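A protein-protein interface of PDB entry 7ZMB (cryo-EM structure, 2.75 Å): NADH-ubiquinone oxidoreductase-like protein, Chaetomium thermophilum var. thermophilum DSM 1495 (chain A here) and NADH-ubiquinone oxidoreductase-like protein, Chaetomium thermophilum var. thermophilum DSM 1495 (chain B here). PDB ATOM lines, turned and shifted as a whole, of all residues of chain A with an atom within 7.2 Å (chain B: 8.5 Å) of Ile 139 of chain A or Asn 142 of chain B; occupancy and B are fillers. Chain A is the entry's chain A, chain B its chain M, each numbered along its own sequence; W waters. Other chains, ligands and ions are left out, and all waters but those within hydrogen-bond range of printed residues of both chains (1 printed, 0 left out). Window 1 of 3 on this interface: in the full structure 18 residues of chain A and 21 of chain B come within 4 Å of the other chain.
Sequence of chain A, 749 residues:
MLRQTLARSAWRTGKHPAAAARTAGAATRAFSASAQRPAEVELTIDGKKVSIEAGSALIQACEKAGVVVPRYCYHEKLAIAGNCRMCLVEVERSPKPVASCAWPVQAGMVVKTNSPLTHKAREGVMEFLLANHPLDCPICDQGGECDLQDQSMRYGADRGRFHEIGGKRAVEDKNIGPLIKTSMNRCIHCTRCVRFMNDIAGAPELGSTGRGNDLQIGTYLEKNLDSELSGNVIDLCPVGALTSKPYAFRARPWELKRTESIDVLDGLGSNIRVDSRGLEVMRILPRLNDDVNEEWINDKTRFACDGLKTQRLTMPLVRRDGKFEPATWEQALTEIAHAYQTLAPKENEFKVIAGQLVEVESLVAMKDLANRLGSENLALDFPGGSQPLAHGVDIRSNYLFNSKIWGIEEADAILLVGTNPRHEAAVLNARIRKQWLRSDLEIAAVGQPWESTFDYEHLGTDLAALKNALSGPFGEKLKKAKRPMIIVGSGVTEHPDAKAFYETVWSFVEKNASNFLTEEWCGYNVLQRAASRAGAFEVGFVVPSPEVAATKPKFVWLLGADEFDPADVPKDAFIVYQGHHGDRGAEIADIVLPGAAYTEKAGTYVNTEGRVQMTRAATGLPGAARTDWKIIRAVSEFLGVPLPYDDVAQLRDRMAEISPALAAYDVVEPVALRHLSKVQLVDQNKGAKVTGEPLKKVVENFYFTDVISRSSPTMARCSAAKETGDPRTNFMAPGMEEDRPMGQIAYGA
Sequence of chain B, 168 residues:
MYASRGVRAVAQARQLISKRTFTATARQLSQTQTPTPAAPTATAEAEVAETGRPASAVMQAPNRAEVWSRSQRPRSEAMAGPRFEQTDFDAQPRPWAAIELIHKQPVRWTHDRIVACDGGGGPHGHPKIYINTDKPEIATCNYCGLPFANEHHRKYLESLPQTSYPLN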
ATOM      1  N   LEU A 135      12.647  17.884 -11.936  1.00  0.00           N
ATOM      2  CA  LEU A 135      12.919  18.953 -12.939  1.00  0.00           C
ATOM      3  C   LEU A 135      14.357  19.432 -12.748  1.00  0.00           C
ATOM      4  O   LEU A 135      14.561  20.578 -12.420  1.00  0.00           O
ATOM      5  CB  LEU A 135      11.899  20.088 -12.837  1.00  0.00           C
ATOM      6  CG  LEU A 135      10.692  19.981 -13.765  1.00  0.00           C
ATOM      7  CD1 LEU A 135       9.712  18.933 -13.273  1.00  0.00           C
ATOM      8  CD2 LEU A 135      10.006  21.327 -13.896  1.00  0.00           C
ATOM      9  N   ASP A 136      15.313  18.559 -13.031  1.00  0.00           N
ATOM     10  CA  ASP A 136      16.729  18.855 -12.777  1.00  0.00           C
ATOM     11  C   ASP A 136      17.518  18.742 -14.059  1.00  0.00           C
ATOM     12  O   ASP A 136      18.680  18.331 -13.952  1.00  0.00           O
ATOM     13  CB  ASP A 136      17.331  17.721 -11.958  1.00  0.00           C
ATOM     14  CG  ASP A 136      16.942  17.673 -10.500  1.00  0.00           C
ATOM     15  OD1 ASP A 136      16.063  18.433 -10.092  1.00  0.00           O
ATOM     16  OD2 ASP A 136      17.540  16.868  -9.792  1.00  0.00           O
ATOM     17  N   CYS A 137      16.972  19.127 -15.211  1.00  0.00           N
ATOM     18  CA  CYS A 137      17.749  18.908 -16.467  1.00  0.00           C
ATOM     19  C   CYS A 137      18.843  19.961 -16.501  1.00  0.00           C
ATOM     20  O   CYS A 137      19.891  19.622 -17.000  1.00  0.00           O
ATOM     21  CB  CYS A 137      16.883  19.010 -17.724  1.00  0.00           C
ATOM     22  SG  CYS A 137      15.901  17.539 -18.077  1.00  0.00           S
ATOM     23  N   PRO A 138      18.649  21.232 -16.054  1.00  0.00           N
ATOM     24  CA  PRO A 138      19.776  22.169 -15.946  1.00  0.00           C
ATOM     25  C   PRO A 138      20.947  21.771 -15.029  1.00  0.00           C
ATOM     26  O   PRO A 138      22.047  22.025 -15.400  1.00  0.00           O
ATOM     27  CB  PRO A 138      19.048  23.442 -15.516  1.00  0.00           C
ATOM     28  CG  PRO A 138      17.720  23.332 -16.171  1.00  0.00           C
ATOM     29  CD  PRO A 138      17.369  21.912 -15.824  1.00  0.00           C
ATOM     30  N   ILE A 139      20.706  21.149 -13.879  1.00  0.00           N
ATOM     31  CA  ILE A 139      21.784  20.779 -12.897  1.00  0.00           C
ATOM     32  C   ILE A 139      22.317  19.345 -13.099  1.00  0.00           C
ATOM     33  O   ILE A 139      23.194  18.962 -12.339  1.00  0.00           O
ATOM     34  CB  ILE A 139      21.278  20.994 -11.454  1.00  0.00           C
ATOM     35  CG1 ILE A 139      19.903  20.358 -11.247  1.00  0.00           C
ATOM     36  CG2 ILE A 139      21.287  22.463 -11.073  1.00  0.00           C
ATOM     37  CD1 ILE A 139      19.410  20.398  -9.830  1.00  0.00           C
ATOM     38  N   CYS A 140      21.816  18.586 -14.073  1.00  0.00           N
ATOM     39  CA  CYS A 140      22.181  17.160 -14.310  1.00  0.00           C
ATOM     40  C   CYS A 140      23.322  17.063 -15.313  1.00  0.00           C
ATOM     41  O   CYS A 140      23.323  17.827 -16.267  1.00  0.00           O
ATOM     42  CB  CYS A 140      20.985  16.433 -14.931  1.00  0.00           C
ATOM     43  SG  CYS A 140      21.053  14.629 -14.994  1.00  0.00           S
ATOM     44  N   ASP A 141      24.220  16.101 -15.120  1.00  0.00           N
ATOM     45  CA  ASP A 141      25.393  15.952 -16.011  1.00  0.00           C
ATOM     46  C   ASP A 141      25.050  15.037 -17.179  1.00  0.00           C
ATOM     47  O   ASP A 141      25.921  14.795 -18.005  1.00  0.00           O
ATOM     48  CB  ASP A 141      26.638  15.518 -15.243  1.00  0.00           C
ATOM     49  CG  ASP A 141      27.297  16.633 -14.462  1.00  0.00           C
ATOM     50  OD1 ASP A 141      27.355  17.756 -14.981  1.00  0.00           O
ATOM     51  OD2 ASP A 141      27.738  16.364 -13.342  1.00  0.00           O
ATOM     52  N   GLN A 142      23.829  14.541 -17.253  1.00  0.00           N
ATOM     53  CA  GLN A 142      23.439  13.727 -18.419  1.00  0.00           C
ATOM     54  C   GLN A 142      22.794  14.590 -19.510  1.00  0.00           C
ATOM     55  O   GLN A 142      22.469  14.023 -20.552  1.00  0.00           O
ATOM     56  CB  GLN A 142      22.542  12.591 -17.933  1.00  0.00           C
ATOM     57  CG  GLN A 142      22.178  11.558 -18.990  1.00  0.00           C
ATOM     58  CD  GLN A 142      23.147  10.408 -19.016  1.00  0.00           C
ATOM     59  OE1 GLN A 142      23.532   9.891 -17.978  1.00  0.00           O
ATOM     60  NE2 GLN A 142      23.540   9.989 -20.203  1.00  0.00           N
ATOM     61  N   GLY A 143      22.736  15.914 -19.365  1.00  0.00           N
ATOM     62  CA  GLY A 143      21.978  16.751 -20.322  1.00  0.00           C
ATOM     63  C   GLY A 143      22.683  16.987 -21.634  1.00  0.00           C
ATOM     64  O   GLY A 143      23.818  17.439 -21.597  1.00  0.00           O
ATOM     65  N   ASP A 173      19.710  10.407  -1.103  1.00  0.00           N
ATOM     66  CA  ASP A 173      20.872   9.997  -1.870  1.00  0.00           C
ATOM     67  C   ASP A 173      21.679   8.961  -1.098  1.00  0.00           C
ATOM     68  O   ASP A 173      21.389   8.637   0.052  1.00  0.00           O
ATOM     69  CB  ASP A 173      21.722  11.201  -2.241  1.00  0.00           C
ATOM     70  CG  ASP A 173      21.249  11.859  -3.514  1.00  0.00           C
ATOM     71  OD1 ASP A 173      20.580  11.172  -4.312  1.00  0.00           O
ATOM     72  OD2 ASP A 173      21.546  13.055  -3.719  1.00  0.00           O
ATOM     73  N   LYS A 181      28.956   9.664  -7.938  1.00  0.00           N
ATOM     74  CA  LYS A 181      28.017  10.593  -7.331  1.00  0.00           C
ATOM     75  C   LYS A 181      26.591  10.121  -7.583  1.00  0.00           C
ATOM     76  O   LYS A 181      26.258   9.626  -8.661  1.00  0.00           O
ATOM     77  CB  LYS A 181      28.222  12.006  -7.876  1.00  0.00           C
ATOM     78  CG  LYS A 181      27.185  13.009  -7.408  1.00  0.00           C
ATOM     79  CD  LYS A 181      27.639  14.433  -7.635  1.00  0.00           C
ATOM     80  CE  LYS A 181      26.480  15.422  -7.527  1.00  0.00           C
ATOM     81  NZ  LYS A 181      25.521  15.376  -8.662  1.00  0.00           N
ATOM     82  N   SER A 183      22.412  10.867  -7.326  1.00  0.00           N
ATOM     83  CA  SER A 183      21.243  11.794  -7.384  1.00  0.00           C
ATOM     84  C   SER A 183      20.092  10.862  -7.743  1.00  0.00           C
ATOM     85  O   SER A 183      19.688  10.889  -8.896  1.00  0.00           O
ATOM     86  CB  SER A 183      21.343  12.906  -8.382  1.00  0.00           C
ATOM     87  OG  SER A 183      20.556  14.008  -7.976  1.00  0.00           O
ATOM     88  N   ARG A 186      16.441  10.894  -9.881  1.00  0.00           N
ATOM     89  CA  ARG A 186      16.442  10.736 -11.358  1.00  0.00           C
ATOM     90  C   ARG A 186      16.175   9.294 -11.802  1.00  0.00           C
ATOM     91  O   ARG A 186      15.799   9.124 -12.965  1.00  0.00           O
ATOM     92  CB  ARG A 186      17.742  11.327 -11.907  1.00  0.00           C
ATOM     93  CG  ARG A 186      17.973  12.778 -11.525  1.00  0.00           C
ATOM     94  CD  ARG A 186      19.378  13.247 -11.818  1.00  0.00           C
ATOM     95  NE  ARG A 186      19.568  14.562 -11.236  1.00  0.00           N
ATOM     96  CZ  ARG A 186      20.732  15.183 -11.151  1.00  0.00           C
ATOM     97  NH1 ARG A 186      21.823  14.595 -11.604  1.00  0.00           N
ATOM     98  NH2 ARG A 186      20.800  16.377 -10.597  1.00  0.00           N
ATOM     99  N   PHE A 249      29.828  18.495 -13.105  1.00  0.00           N
ATOM    100  CA  PHE A 249      29.496  19.874 -13.429  1.00  0.00           C
ATOM    101  C   PHE A 249      30.533  20.533 -14.334  1.00  0.00           C
ATOM    102  O   PHE A 249      30.377  21.706 -14.654  1.00  0.00           O
ATOM    103  CB  PHE A 249      29.308  20.763 -12.182  1.00  0.00           C
ATOM    104  CG  PHE A 249      28.483  20.136 -11.090  1.00  0.00           C
ATOM    105  CD1 PHE A 249      27.460  19.261 -11.378  1.00  0.00           C
ATOM    106  CD2 PHE A 249      28.754  20.420  -9.769  1.00  0.00           C
ATOM    107  CE1 PHE A 249      26.719  18.706 -10.381  1.00  0.00           C
ATOM    108  CE2 PHE A 249      28.014  19.855  -8.769  1.00  0.00           C
ATOM    109  CZ  PHE A 249      26.995  18.997  -9.076  1.00  0.00           C
ATOM    110  N   ARG A 252      29.756  19.997 -20.594  1.00  0.00           N
ATOM    111  CA  ARG A 252      28.577  19.560 -21.303  1.00  0.00           C
ATOM    112  C   ARG A 252      28.991  18.773 -22.542  1.00  0.00           C
ATOM    113  O   ARG A 252      30.084  18.982 -23.070  1.00  0.00           O
ATOM    114  CB  ARG A 252      27.706  20.752 -21.707  1.00  0.00           C
ATOM    115  CG  ARG A 252      26.877  21.288 -20.591  1.00  0.00           C
ATOM    116  CD  ARG A 252      25.850  20.293 -20.152  1.00  0.00           C
ATOM    117  NE  ARG A 252      24.974  20.858 -19.136  1.00  0.00           N
ATOM    118  CZ  ARG A 252      24.063  20.172 -18.465  1.00  0.00           C
ATOM    119  NH1 ARG A 252      23.899  18.883 -18.696  1.00  0.00           N
ATOM    120  NH2 ARG A 252      23.314  20.779 -17.569  1.00  0.00           N
ATOM    121  N   CYS B 117      10.580  23.018  -3.271  1.00  0.00           N
ATOM    122  CA  CYS B 117      11.190  24.328  -3.427  1.00  0.00           C
ATOM    123  C   CYS B 117      11.109  24.736  -4.886  1.00  0.00           C
ATOM    124  O   CYS B 117      11.521  23.983  -5.771  1.00  0.00           O
ATOM    125  CB  CYS B 117      12.645  24.344  -2.950  1.00  0.00           C
ATOM    126  SG  CYS B 117      13.311  26.001  -2.726  1.00  0.00           S
ATOM    127  N   HIS B 126      12.824  29.236  -9.666  1.00  0.00           N
ATOM    128  CA  HIS B 126      13.544  28.206 -10.399  1.00  0.00           C
ATOM    129  C   HIS B 126      12.599  27.032 -10.648  1.00  0.00           C
ATOM    130  O   HIS B 126      11.474  27.047 -10.140  1.00  0.00           O
ATOM    131  CB  HIS B 126      14.821  27.805  -9.640  1.00  0.00           C
ATOM    132  CG  HIS B 126      14.587  27.159  -8.310  1.00  0.00           C
ATOM    133  ND1 HIS B 126      13.849  26.009  -8.154  1.00  0.00           N
ATOM    134  CD2 HIS B 126      15.025  27.492  -7.077  1.00  0.00           C
ATOM    135  CE1 HIS B 126      13.832  25.668  -6.881  1.00  0.00           C
ATOM    136  NE2 HIS B 126      14.533  26.556  -6.204  1.00  0.00           N
ATOM    137  N   PRO B 127      12.982  26.033 -11.449  1.00  0.00           N
ATOM    138  CA  PRO B 127      12.102  24.871 -11.644  1.00  0.00           C
ATOM    139  C   PRO B 127      11.791  24.165 -10.334  1.00  0.00           C
ATOM    140  O   PRO B 127      12.672  23.937  -9.509  1.00  0.00           O
ATOM    141  CB  PRO B 127      12.912  23.978 -12.587  1.00  0.00           C
ATOM    142  CG  PRO B 127      13.824  24.895 -13.275  1.00  0.00           C
ATOM    143  CD  PRO B 127      14.198  25.918 -12.275  1.00  0.00           C
ATOM    144  N   ILE B 129      11.239  21.540  -7.588  1.00  0.00           N
ATOM    145  CA  ILE B 129      11.816  20.241  -7.275  1.00  0.00           C
ATOM    146  C   ILE B 129      11.366  19.821  -5.887  1.00  0.00           C
ATOM    147  O   ILE B 129      10.635  20.532  -5.202  1.00  0.00           O
ATOM    148  CB  ILE B 129      13.356  20.234  -7.362  1.00  0.00           C
ATOM    149  CG1 ILE B 129      13.943  21.223  -6.360  1.00  0.00           C
ATOM    150  CG2 ILE B 129      13.821  20.463  -8.797  1.00  0.00           C
ATOM    151  CD1 ILE B 129      15.408  21.113  -6.208  1.00  0.00           C
ATOM    152  N   TYR B 130      11.823  18.645  -5.476  1.00  0.00           N
ATOM    153  CA  TYR B 130      11.402  18.024  -4.232  1.00  0.00           C
ATOM    154  C   TYR B 130      12.624  17.481  -3.521  1.00  0.00           C
ATOM    155  O   TYR B 130      13.461  16.822  -4.142  1.00  0.00           O
ATOM    156  CB  TYR B 130      10.389  16.913  -4.502  1.00  0.00           C
ATOM    157  CG  TYR B 130       9.126  17.452  -5.106  1.00  0.00           C
ATOM    158  CD1 TYR B 130       8.131  17.993  -4.308  1.00  0.00           C
ATOM    159  CD2 TYR B 130       8.955  17.481  -6.480  1.00  0.00           C
ATOM    160  CE1 TYR B 130       6.992  18.510  -4.857  1.00  0.00           C
ATOM    161  CE2 TYR B 130       7.821  18.004  -7.038  1.00  0.00           C
ATOM    162  CZ  TYR B 130       6.836  18.514  -6.220  1.00  0.00           C
ATOM    163  OH  TYR B 130       5.689  19.030  -6.759  1.00  0.00           O
ATOM    164  N   ILE B 131      12.736  17.753  -2.227  1.00  0.00           N
ATOM    165  CA  ILE B 131      13.896  17.343  -1.454  1.00  0.00           C
ATOM    166  C   ILE B 131      13.431  16.368  -0.383  1.00  0.00           C
ATOM    167  O   ILE B 131      12.552  16.689   0.424  1.00  0.00           O
ATOM    168  CB  ILE B 131      14.630  18.537  -0.823  1.00  0.00           C
ATOM    169  CG1 ILE B 131      15.155  19.504  -1.884  1.00  0.00           C
ATOM    170  CG2 ILE B 131      15.790  18.052  -0.018  1.00  0.00           C
ATOM    171  CD1 ILE B 131      14.203  20.596  -2.257  1.00  0.00           C
ATOM    172  N   ASN B 132      14.017  15.177  -0.388  1.00  0.00           N
ATOM    173  CA  ASN B 132      13.816  14.206   0.677  1.00  0.00           C
ATOM    174  C   ASN B 132      14.566  14.651   1.929  1.00  0.00           C
ATOM    175  O   ASN B 132      15.716  15.091   1.852  1.00  0.00           O
ATOM    176  CB  ASN B 132      14.299  12.834   0.204  1.00  0.00           C
ATOM    177  CG  ASN B 132      13.941  11.711   1.153  1.00  0.00           C
ATOM    178  OD1 ASN B 132      14.711  11.373   2.045  1.00  0.00           O
ATOM    179  ND2 ASN B 132      12.773  11.122   0.958  1.00  0.00           N
ATOM    180  N   ALA B 139      19.087  18.986   4.604  1.00  0.00           N
ATOM    181  CA  ALA B 139      18.862  18.819   3.177  1.00  0.00           C
ATOM    182  C   ALA B 139      18.810  20.169   2.480  1.00  0.00           C
ATOM    183  O   ALA B 139      18.130  21.092   2.927  1.00  0.00           O
ATOM    184  CB  ALA B 139      17.572  18.053   2.934  1.00  0.00           C
ATOM    185  N   THR B 140      19.528  20.273   1.375  1.00  0.00           N
ATOM    186  CA  THR B 140      19.732  21.526   0.666  1.00  0.00           C
ATOM    187  C   THR B 140      19.081  21.452  -0.707  1.00  0.00           C
ATOM    188  O   THR B 140      19.127  20.414  -1.367  1.00  0.00           O
ATOM    189  CB  THR B 140      21.240  21.824   0.527  1.00  0.00           C
ATOM    190  OG1 THR B 140      21.849  21.871   1.824  1.00  0.00           O
ATOM    191  CG2 THR B 140      21.467  23.123  -0.157  1.00  0.00           C
ATOM    192  N   CYS B 141      18.473  22.554  -1.132  1.00  0.00           N
ATOM    193  CA  CYS B 141      17.951  22.649  -2.487  1.00  0.00           C
ATOM    194  C   CYS B 141      19.101  22.794  -3.476  1.00  0.00           C
ATOM    195  O   CYS B 141      19.994  23.624  -3.290  1.00  0.00           O
ATOM    196  CB  CYS B 141      16.991  23.831  -2.598  1.00  0.00           C
ATOM    197  SG  CYS B 141      16.178  24.050  -4.203  1.00  0.00           S
ATOM    198  N   ASN B 142      19.082  21.985  -4.529  1.00  0.00           N
ATOM    199  CA  ASN B 142      20.185  21.976  -5.478  1.00  0.00           C
ATOM    200  C   ASN B 142      20.235  23.226  -6.339  1.00  0.00           C
ATOM    201  O   ASN B 142      21.293  23.538  -6.889  1.00  0.00           O
ATOM    202  CB  ASN B 142      20.097  20.749  -6.373  1.00  0.00           C
ATOM    203  CG  ASN B 142      20.695  19.528  -5.740  1.00  0.00           C
ATOM    204  OD1 ASN B 142      20.154  18.982  -4.784  1.00  0.00           O
ATOM    205  ND2 ASN B 142      21.820  19.082  -6.271  1.00  0.00           N
ATOM    206  N   TYR B 143      19.130  23.954  -6.464  1.00  0.00           N
ATOM    207  CA  TYR B 143      19.132  25.186  -7.243  1.00  0.00           C
ATOM    208  C   TYR B 143      19.572  26.389  -6.413  1.00  0.00           C
ATOM    209  O   TYR B 143      20.516  27.088  -6.782  1.00  0.00           O
ATOM    210  CB  TYR B 143      17.748  25.432  -7.849  1.00  0.00           C
ATOM    211  CG  TYR B 143      17.449  24.639  -9.095  1.00  0.00           C
ATOM    212  CD1 TYR B 143      17.909  25.053 -10.323  1.00  0.00           C
ATOM    213  CD2 TYR B 143      16.681  23.489  -9.043  1.00  0.00           C
ATOM    214  CE1 TYR B 143      17.628  24.344 -11.464  1.00  0.00           C
ATOM    215  CE2 TYR B 143      16.398  22.776 -10.177  1.00  0.00           C
ATOM    216  CZ  TYR B 143      16.877  23.211 -11.390  1.00  0.00           C
ATOM    217  OH  TYR B 143      16.607  22.511 -12.538  1.00  0.00           O
ATOM    218  N   CYS B 144      18.953  26.602  -5.252  1.00  0.00           N
ATOM    219  CA  CYS B 144      19.208  27.856  -4.483  1.00  0.00           C
ATOM    220  C   CYS B 144      19.959  27.656  -3.167  1.00  0.00           C
ATOM    221  O   CYS B 144      20.389  28.661  -2.605  1.00  0.00           O
ATOM    222  CB  CYS B 144      17.907  28.609  -4.226  1.00  0.00           C
ATOM    223  SG  CYS B 144      16.681  27.748  -3.210  1.00  0.00           S
ATOM    224  N   GLY B 145      20.118  26.430  -2.689  1.00  0.00           N
ATOM    225  CA  GLY B 145      20.922  26.229  -1.477  1.00  0.00           C
ATOM    226  C   GLY B 145      20.132  26.410  -0.197  1.00  0.00           C
ATOM    227  O   GLY B 145      20.764  26.339   0.866  1.00  0.00           O
ATOM    228  N   LEU B 146      18.821  26.651  -0.266  1.00  0.00           N
ATOM    229  CA  LEU B 146      18.115  26.861   0.987  1.00  0.00           C
ATOM    230  C   LEU B 146      18.124  25.587   1.826  1.00  0.00           C
ATOM    231  O   LEU B 146      17.931  24.492   1.297  1.00  0.00           O
ATOM    232  CB  LEU B 146      16.678  27.295   0.739  1.00  0.00           C
ATOM    233  CG  LEU B 146      16.416  28.784   0.568  1.00  0.00           C
ATOM    234  CD1 LEU B 146      14.938  29.048   0.715  1.00  0.00           C
ATOM    235  CD2 LEU B 146      17.220  29.602   1.553  1.00  0.00           C
ATOM    236  N   PHE B 148      16.890  22.735   4.498  1.00  0.00           N
ATOM    237  CA  PHE B 148      15.750  22.104   5.144  1.00  0.00           C
ATOM    238  C   PHE B 148      16.229  21.010   6.079  1.00  0.00           C
ATOM    239  O   PHE B 148      17.252  20.364   5.839  1.00  0.00           O
ATOM    240  CB  PHE B 148      14.761  21.505   4.141  1.00  0.00           C
ATOM    241  CG  PHE B 148      14.282  22.467   3.117  1.00  0.00           C
ATOM    242  CD1 PHE B 148      14.996  22.680   1.962  1.00  0.00           C
ATOM    243  CD2 PHE B 148      13.103  23.158   3.302  1.00  0.00           C
ATOM    244  CE1 PHE B 148      14.550  23.577   1.024  1.00  0.00           C
ATOM    245  CE2 PHE B 148      12.658  24.051   2.358  1.00  0.00           C
ATOM    246  CZ  PHE B 148      13.383  24.256   1.220  1.00  0.00           C
HETATM  247  O   HOH W   1      19.072  17.114  -7.533  1.00  0.00           O
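Pro 127 of chain B touches Leu 135 of chain A (CB to O, 3.8 Å).
O of Leu 135 of chain A touches CG2 of Ile 129 of chain B (3.7 Å).
OD1 of Asp 136 of chain A touches CG2 of Ile 129 of chain B, 3.3 Å away.
Asp 136 of chain A touches Tyr 143 of chain B.
Tyr 143 of chain B touches Pro 138 of chain A.
Asn 142 of chain B touches Ile 139 of chain A.
Ile 139 of chain A touches Tyr 143 of chain B.
The backbone NH of Tyr 143 of chain B lies close to the side-chain sulfur of Cys 141 of chain B (3.7 Å).
The guanidinium group of Arg 186 of chain A lies within salt-bridge range of the side-chain carboxylate of Asp 136 of chain A (3.4 Å).
The backbone carbonyl oxygen (O) of Pro 138 of chain A lies within hydrogen-bond range of the guanidinium group (NH2) of Arg 252 of chain A (2.8 Å).
The backbone NH (N) of Ile 129 of chain B is in hydrogen-bond range of the backbone carbonyl oxygen (O) of Cys 117 of chain B (3.1 Å).
Hydrophobic or aromatic side chains of chain B within 4 Å of the printed part of chain A: Pro 127, Ile 129 and Tyr 143.
Along chain B the printed residues that touch a printed residue of chain A span positions 127 to 143.
Of the 15 printed residues of chain A, 4 touch a printed residue of chain B.
Hydrophobic or aromatic side chains of chain A within 4 Å of the printed part of chain B: Pro 138 and Ile 139.
Along chain A the printed residues that touch a printed residue of chain B span positions 135 to 139.
Of the printed residues of chain B, Leu 135 of chain A touches Pro 127 (3.8 Å), Ile 129 (3.7 Å) and Tyr 143 (2.8 Å).
Printed residues of chain B within 4 Å of Asp 136 of chain A: Ile 129 and Tyr 143.
Pro 138 of chain A touches just one residue of chain B: Tyr 143.
Ile 139 of chain A touches just these residues of chain B: Asn 142 (3.5 Å) and Tyr 143 (3.9 Å).
Printed residues of chain A within 4 Å of Pro 127 of chain B: Leu 135 (3.8 Å).
Printed residues of chain A within 4 Å of Ile 129 of chain B: Leu 135 and Asp 136.
Asn 132 of chain B touches none of the printed residues of chain A.
Printed residues of chain A within 4 Å of Asn 142 of chain B: Ile 139.
Of the printed residues of chain A, Tyr 143 of chain B touches Leu 135 (2.8 Å), Asp 136 (3.7 Å), Pro 138 (3.4 Å) and Ile 139 (3.9 Å).
The nearest residue of chain A that does not touch Asn 142 of chain B is Arg 186 of chain A (5.2 Å).
The side-chain hydroxyl of Tyr 143 of chain B sits at hydrogen-bond distance from the backbone carbonyl oxygen of Leu 135 of chain A, 2.8 Å away.
Water W1 lies within hydrogen-bond range of the side-chain carboxylate of Asp 136 of chain A (2.7 Å), the side-chain hydroxyl of Ser 183 of chain A (3.5 Å) and the side-chain amide oxygen of Asn 142 of chain B (3.5 Å).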
